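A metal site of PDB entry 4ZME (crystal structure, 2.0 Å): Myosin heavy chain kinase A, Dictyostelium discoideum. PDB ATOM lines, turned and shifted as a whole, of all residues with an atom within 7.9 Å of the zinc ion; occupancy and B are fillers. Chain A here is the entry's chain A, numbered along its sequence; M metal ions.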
ATOM      1  N   SER A 201       8.910   5.137   2.022  1.00  0.00           N
ATOM      2  CA  SER A 201       9.878   4.111   2.383  1.00  0.00           C
ATOM      3  C   SER A 201      11.281   4.354   1.797  1.00  0.00           C
ATOM      4  O   SER A 201      12.272   4.178   2.494  1.00  0.00           O
ATOM      5  CB  SER A 201       9.359   2.749   1.908  1.00  0.00           C
ATOM      6  OG  SER A 201       8.313   2.302   2.743  1.00  0.00           O
ATOM      7  N   GLN A 204      14.066   6.562   3.515  1.00  0.00           N
ATOM      8  CA  GLN A 204      14.586   6.000   4.741  1.00  0.00           C
ATOM      9  C   GLN A 204      15.408   4.765   4.455  1.00  0.00           C
ATOM     10  O   GLN A 204      16.431   4.508   5.121  1.00  0.00           O
ATOM     11  CB  GLN A 204      13.442   5.704   5.729  1.00  0.00           C
ATOM     12  CG  GLN A 204      12.450   6.853   5.886  1.00  0.00           C
ATOM     13  CD  GLN A 204      13.059   8.168   6.339  1.00  0.00           C
ATOM     14  OE1 GLN A 204      14.072   8.200   7.041  1.00  0.00           O
ATOM     15  NE2 GLN A 204      12.418   9.279   5.943  1.00  0.00           N
ATOM     16  N   ALA A 205      15.002   3.967   3.473  1.00  0.00           N
ATOM     17  CA  ALA A 205      15.763   2.803   3.099  1.00  0.00           C
ATOM     18  C   ALA A 205      17.146   3.226   2.520  1.00  0.00           C
ATOM     19  O   ALA A 205      18.177   2.575   2.728  1.00  0.00           O
ATOM     20  CB  ALA A 205      15.008   1.982   2.054  1.00  0.00           C
ATOM     21  N   PHE A 206      17.139   4.295   1.761  1.00  0.00           N
ATOM     22  CA  PHE A 206      18.367   4.770   1.164  1.00  0.00           C
ATOM     23  C   PHE A 206      19.311   5.200   2.299  1.00  0.00           C
ATOM     24  O   PHE A 206      20.482   4.825   2.270  1.00  0.00           O
ATOM     25  CB  PHE A 206      18.122   5.913   0.200  1.00  0.00           C
ATOM     26  CG  PHE A 206      19.391   6.580  -0.244  1.00  0.00           C
ATOM     27  CD1 PHE A 206      20.232   5.961  -1.138  1.00  0.00           C
ATOM     28  CD2 PHE A 206      19.776   7.790   0.293  1.00  0.00           C
ATOM     29  CE1 PHE A 206      21.418   6.549  -1.528  1.00  0.00           C
ATOM     30  CE2 PHE A 206      20.951   8.407  -0.098  1.00  0.00           C
ATOM     31  CZ  PHE A 206      21.785   7.778  -1.014  1.00  0.00           C
ATOM     32  N   SER A 207      18.818   5.948   3.267  1.00  0.00           N
ATOM     33  CA  SER A 207      19.673   6.356   4.410  1.00  0.00           C
ATOM     34  C   SER A 207      20.276   5.123   5.116  1.00  0.00           C
ATOM     35  O   SER A 207      21.515   5.067   5.376  1.00  0.00           O
ATOM     36  CB  SER A 207      18.929   7.254   5.397  1.00  0.00           C
ATOM     37  OG  SER A 207      18.632   8.516   4.812  1.00  0.00           O
ATOM     38  N   HIS A 208      19.443   4.128   5.376  1.00  0.00           N
ATOM     39  CA  HIS A 208      19.911   2.870   5.993  1.00  0.00           C
ATOM     40  C   HIS A 208      20.976   2.173   5.109  1.00  0.00           C
ATOM     41  O   HIS A 208      21.994   1.712   5.618  1.00  0.00           O
ATOM     42  CB  HIS A 208      18.721   1.924   6.301  1.00  0.00           C
ATOM     43  CG  HIS A 208      19.089   0.701   7.090  1.00  0.00           C
ATOM     44  ND1 HIS A 208      18.187  -0.305   7.362  1.00  0.00           N
ATOM     45  CD2 HIS A 208      20.258   0.301   7.643  1.00  0.00           C
ATOM     46  CE1 HIS A 208      18.773  -1.254   8.061  1.00  0.00           C
ATOM     47  NE2 HIS A 208      20.039  -0.927   8.230  1.00  0.00           N
ATOM     48  N   PHE A 209      20.693   2.052   3.814  1.00  0.00           N
ATOM     49  CA  PHE A 209      21.581   1.439   2.833  1.00  0.00           C
ATOM     50  C   PHE A 209      22.961   2.086   2.902  1.00  0.00           C
ATOM     51  O   PHE A 209      23.954   1.384   2.939  1.00  0.00           O
ATOM     52  CB  PHE A 209      20.981   1.621   1.427  1.00  0.00           C
ATOM     53  CG  PHE A 209      21.862   1.132   0.289  1.00  0.00           C
ATOM     54  CD1 PHE A 209      21.806  -0.201  -0.139  1.00  0.00           C
ATOM     55  CD2 PHE A 209      22.682   2.006  -0.406  1.00  0.00           C
ATOM     56  CE1 PHE A 209      22.569  -0.657  -1.188  1.00  0.00           C
ATOM     57  CE2 PHE A 209      23.428   1.557  -1.472  1.00  0.00           C
ATOM     58  CZ  PHE A 209      23.392   0.224  -1.854  1.00  0.00           C
ATOM     59  N   GLU A 212      24.828   0.909   6.108  1.00  0.00           N
ATOM     60  CA  GLU A 212      25.232  -0.477   6.149  1.00  0.00           C
ATOM     61  C   GLU A 212      26.324  -0.748   5.111  1.00  0.00           C
ATOM     62  O   GLU A 212      27.366  -1.327   5.440  1.00  0.00           O
ATOM     63  CB  GLU A 212      24.050  -1.435   5.944  1.00  0.00           C
ATOM     64  CG  GLU A 212      24.541  -2.872   6.022  1.00  0.00           C
ATOM     65  CD  GLU A 212      23.445  -3.926   6.101  1.00  0.00           C
ATOM     66  OE1 GLU A 212      23.588  -4.950   5.408  1.00  0.00           O
ATOM     67  OE2 GLU A 212      22.477  -3.719   6.862  1.00  0.00           O
ATOM     68  N   PHE A 256      19.616   9.019  13.988  1.00  0.00           N
ATOM     69  CA  PHE A 256      18.940   8.334  12.895  1.00  0.00           C
ATOM     70  C   PHE A 256      18.474   6.931  13.279  1.00  0.00           C
ATOM     71  O   PHE A 256      17.379   6.479  12.895  1.00  0.00           O
ATOM     72  CB  PHE A 256      19.832   8.221  11.655  1.00  0.00           C
ATOM     73  CG  PHE A 256      19.215   7.391  10.569  1.00  0.00           C
ATOM     74  CD1 PHE A 256      18.336   7.953   9.660  1.00  0.00           C
ATOM     75  CD2 PHE A 256      19.498   6.041  10.463  1.00  0.00           C
ATOM     76  CE1 PHE A 256      17.760   7.195   8.672  1.00  0.00           C
ATOM     77  CE2 PHE A 256      18.928   5.275   9.472  1.00  0.00           C
ATOM     78  CZ  PHE A 256      18.064   5.844   8.574  1.00  0.00           C
ATOM     79  N   HIS A 260      14.687   5.138  13.221  1.00  0.00           N
ATOM     80  CA  HIS A 260      14.545   4.354  12.010  1.00  0.00           C
ATOM     81  C   HIS A 260      13.790   3.058  12.258  1.00  0.00           C
ATOM     82  O   HIS A 260      14.133   2.284  13.131  1.00  0.00           O
ATOM     83  CB  HIS A 260      15.899   4.010  11.363  1.00  0.00           C
ATOM     84  CG  HIS A 260      15.784   3.191  10.119  1.00  0.00           C
ATOM     85  ND1 HIS A 260      15.281   3.711   8.951  1.00  0.00           N
ATOM     86  CD2 HIS A 260      16.065   1.895   9.856  1.00  0.00           C
ATOM     87  CE1 HIS A 260      15.289   2.789   8.017  1.00  0.00           C
ATOM     88  NE2 HIS A 260      15.755   1.666   8.537  1.00  0.00           N
ATOM     89  N   LYS A 261      12.777   2.827  11.442  1.00  0.00           N
ATOM     90  CA  LYS A 261      12.045   1.566  11.435  1.00  0.00           C
ATOM     91  C   LYS A 261      12.156   1.005  10.046  1.00  0.00           C
ATOM     92  O   LYS A 261      11.723   1.656   9.099  1.00  0.00           O
ATOM     93  CB  LYS A 261      10.579   1.805  11.758  1.00  0.00           C
ATOM     94  CG  LYS A 261      10.380   2.081  13.227  1.00  0.00           C
ATOM     95  CD  LYS A 261       9.376   3.180  13.451  1.00  0.00           C
ATOM     96  CE  LYS A 261       9.156   3.451  14.933  1.00  0.00           C
ATOM     97  NZ  LYS A 261       7.776   3.976  15.124  1.00  0.00           N
ATOM     98  N   CYS A 262      12.738  -0.174   9.929  1.00  0.00           N
ATOM     99  CA  CYS A 262      12.966  -0.735   8.633  1.00  0.00           C
ATOM    100  C   CYS A 262      11.595  -0.939   7.988  1.00  0.00           C
ATOM    101  O   CYS A 262      10.586  -1.131   8.688  1.00  0.00           O
ATOM    102  CB  CYS A 262      13.738  -2.050   8.700  1.00  0.00           C
ATOM    103  SG  CYS A 262      15.549  -1.928   8.894  1.00  0.00           S
ATOM    104  N   ASN A 263      11.582  -0.829   6.665  1.00  0.00           N
ATOM    105  CA  ASN A 263      10.395  -0.952   5.843  1.00  0.00           C
ATOM    106  C   ASN A 263      10.664  -2.011   4.815  1.00  0.00           C
ATOM    107  O   ASN A 263      11.671  -2.698   4.878  1.00  0.00           O
ATOM    108  CB  ASN A 263      10.045   0.391   5.192  1.00  0.00           C
ATOM    109  CG  ASN A 263      11.200   0.995   4.399  1.00  0.00           C
ATOM    110  OD1 ASN A 263      11.658   0.421   3.426  1.00  0.00           O
ATOM    111  ND2 ASN A 263      11.652   2.196   4.812  1.00  0.00           N
ATOM    112  N   ALA A 264       9.743  -2.186   3.874  1.00  0.00           N
ATOM    113  CA  ALA A 264       9.865  -3.197   2.818  1.00  0.00           C
ATOM    114  C   ALA A 264      11.060  -3.017   1.887  1.00  0.00           C
ATOM    115  O   ALA A 264      11.572  -4.005   1.350  1.00  0.00           O
ATOM    116  CB  ALA A 264       8.600  -3.222   1.990  1.00  0.00           C
ATOM    117  N   VAL A 265      11.448  -1.773   1.637  1.00  0.00           N
ATOM    118  CA  VAL A 265      12.581  -1.545   0.742  1.00  0.00           C
ATOM    119  C   VAL A 265      13.866  -1.955   1.467  1.00  0.00           C
ATOM    120  O   VAL A 265      14.706  -2.562   0.840  1.00  0.00           O
ATOM    121  CB  VAL A 265      12.669  -0.094   0.234  1.00  0.00           C
ATOM    122  CG1 VAL A 265      13.838   0.039  -0.723  1.00  0.00           C
ATOM    123  CG2 VAL A 265      11.370   0.297  -0.459  1.00  0.00           C
ATOM    124  N   CYS A 266      13.973  -1.681   2.768  1.00  0.00           N
ATOM    125  CA  CYS A 266      15.109  -2.176   3.587  1.00  0.00           C
ATOM    126  C   CYS A 266      15.221  -3.690   3.456  1.00  0.00           C
ATOM    127  O   CYS A 266      16.287  -4.220   3.214  1.00  0.00           O
ATOM    128  CB  CYS A 266      14.962  -1.796   5.065  1.00  0.00           C
ATOM    129  SG  CYS A 266      14.974  -0.004   5.451  1.00  0.00           S
ATOM    130  N   ALA A 267      14.109  -4.384   3.609  1.00  0.00           N
ATOM    131  CA  ALA A 267      14.073  -5.841   3.504  1.00  0.00           C
ATOM    132  C   ALA A 267      14.458  -6.303   2.126  1.00  0.00           C
ATOM    133  O   ALA A 267      15.238  -7.242   1.952  1.00  0.00           O
ATOM    134  CB  ALA A 267      12.684  -6.353   3.855  1.00  0.00           C
ATOM    135  N   LEU A 271      18.930  -5.513   3.981  1.00  0.00           N
ATOM    136  CA  LEU A 271      19.570  -4.797   5.050  1.00  0.00           C
ATOM    137  C   LEU A 271      19.228  -5.408   6.393  1.00  0.00           C
ATOM    138  O   LEU A 271      18.105  -5.850   6.623  1.00  0.00           O
ATOM    139  CB  LEU A 271      19.135  -3.330   5.040  1.00  0.00           C
ATOM    140  CG  LEU A 271      19.390  -2.587   3.720  1.00  0.00           C
ATOM    141  CD1 LEU A 271      18.965  -1.146   3.875  1.00  0.00           C
ATOM    142  CD2 LEU A 271      20.837  -2.690   3.304  1.00  0.00           C
ATOM    143  N   ASP A 272      20.195  -5.386   7.292  1.00  0.00           N
ATOM    144  CA  ASP A 272      20.069  -5.918   8.631  1.00  0.00           C
ATOM    145  C   ASP A 272      19.107  -5.046   9.428  1.00  0.00           C
ATOM    146  O   ASP A 272      19.309  -3.843   9.514  1.00  0.00           O
ATOM    147  CB  ASP A 272      21.455  -5.930   9.297  1.00  0.00           C
ATOM    148  CG  ASP A 272      21.558  -6.910  10.449  1.00  0.00           C
ATOM    149  OD1 ASP A 272      20.628  -6.975  11.271  1.00  0.00           O
ATOM    150  OD2 ASP A 272      22.597  -7.597  10.541  1.00  0.00           O
ATOM    151  N   VAL A 273      18.083  -5.636  10.030  1.00  0.00           N
ATOM    152  CA  VAL A 273      17.210  -4.875  10.953  1.00  0.00           C
ATOM    153  C   VAL A 273      17.978  -4.383  12.202  1.00  0.00           C
ATOM    154  O   VAL A 273      17.606  -3.385  12.811  1.00  0.00           O
ATOM    155  CB  VAL A 273      15.943  -5.672  11.384  1.00  0.00           C
ATOM    156  CG1 VAL A 273      15.152  -6.088  10.156  1.00  0.00           C
ATOM    157  CG2 VAL A 273      16.289  -6.899  12.224  1.00  0.00           C
ATOM    158  N   LYS A 274      19.073  -5.055  12.552  1.00  0.00           N
ATOM    159  CA  LYS A 274      19.933  -4.570  13.641  1.00  0.00           C
ATOM    160  C   LYS A 274      20.956  -3.679  12.963  1.00  0.00           C
ATOM    161  O   LYS A 274      21.669  -4.138  12.075  1.00  0.00           O
ATOM    162  CB  LYS A 274      20.599  -5.734  14.380  1.00  0.00           C
ATOM    163  CG  LYS A 274      21.220  -5.332  15.707  1.00  0.00           C
ATOM    164  CD  LYS A 274      22.008  -6.488  16.345  1.00  0.00           C
ATOM    165  CE  LYS A 274      23.005  -5.975  17.390  1.00  0.00           C
ATOM    166  NZ  LYS A 274      24.212  -5.312  16.816  1.00  0.00           N
ATOM    167  N   LEU A 275      20.957  -2.383  13.307  1.00  0.00           N
ATOM    168  CA  LEU A 275      21.877  -1.408  12.703  1.00  0.00           C
ATOM    169  C   LEU A 275      23.305  -1.468  13.286  1.00  0.00           C
ATOM    170  O   LEU A 275      24.295  -1.473  12.551  1.00  0.00           O
ATOM    171  CB  LEU A 275      21.269   0.019  12.702  1.00  0.00           C
ATOM    172  CG  LEU A 275      20.512   0.398  11.410  1.00  0.00           C
ATOM    173  CD1 LEU A 275      19.099  -0.161  11.388  1.00  0.00           C
ATOM    174  CD2 LEU A 275      20.478   1.895  11.206  1.00  0.00           C
HETATM  175 ZN    ZN M   1      16.039  -0.010   7.486  1.00  0.00          ZN
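A ring nitrogen (NE2) of His 208 sits close to the backbone carbonyl oxygen (O) of Asp 272 (3.3 Å).
The backbone NH of Cys 266 lies within hydrogen-bond range of the side-chain amide oxygen of Asn 263 (3.2 Å).
O of Cys 266 is in hydrogen-bond range of N of Leu 271 (3.0 Å).
The zinc ion is bound by NE2 of His 260 (2.0 Å), ND1 of His 208 (2.2 Å), SG of Cys 266 (2.3 Å) and SG of Cys 262 (2.4 Å).
The zinc ion has four donor atoms within binding distance.
Four residues have an atom within 4 Å of the zinc ion: His 208, His 260, Cys 262 and Cys 266.
The nearest printed residue that does not touch the zinc ion is Asn 263 (4.6 Å).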
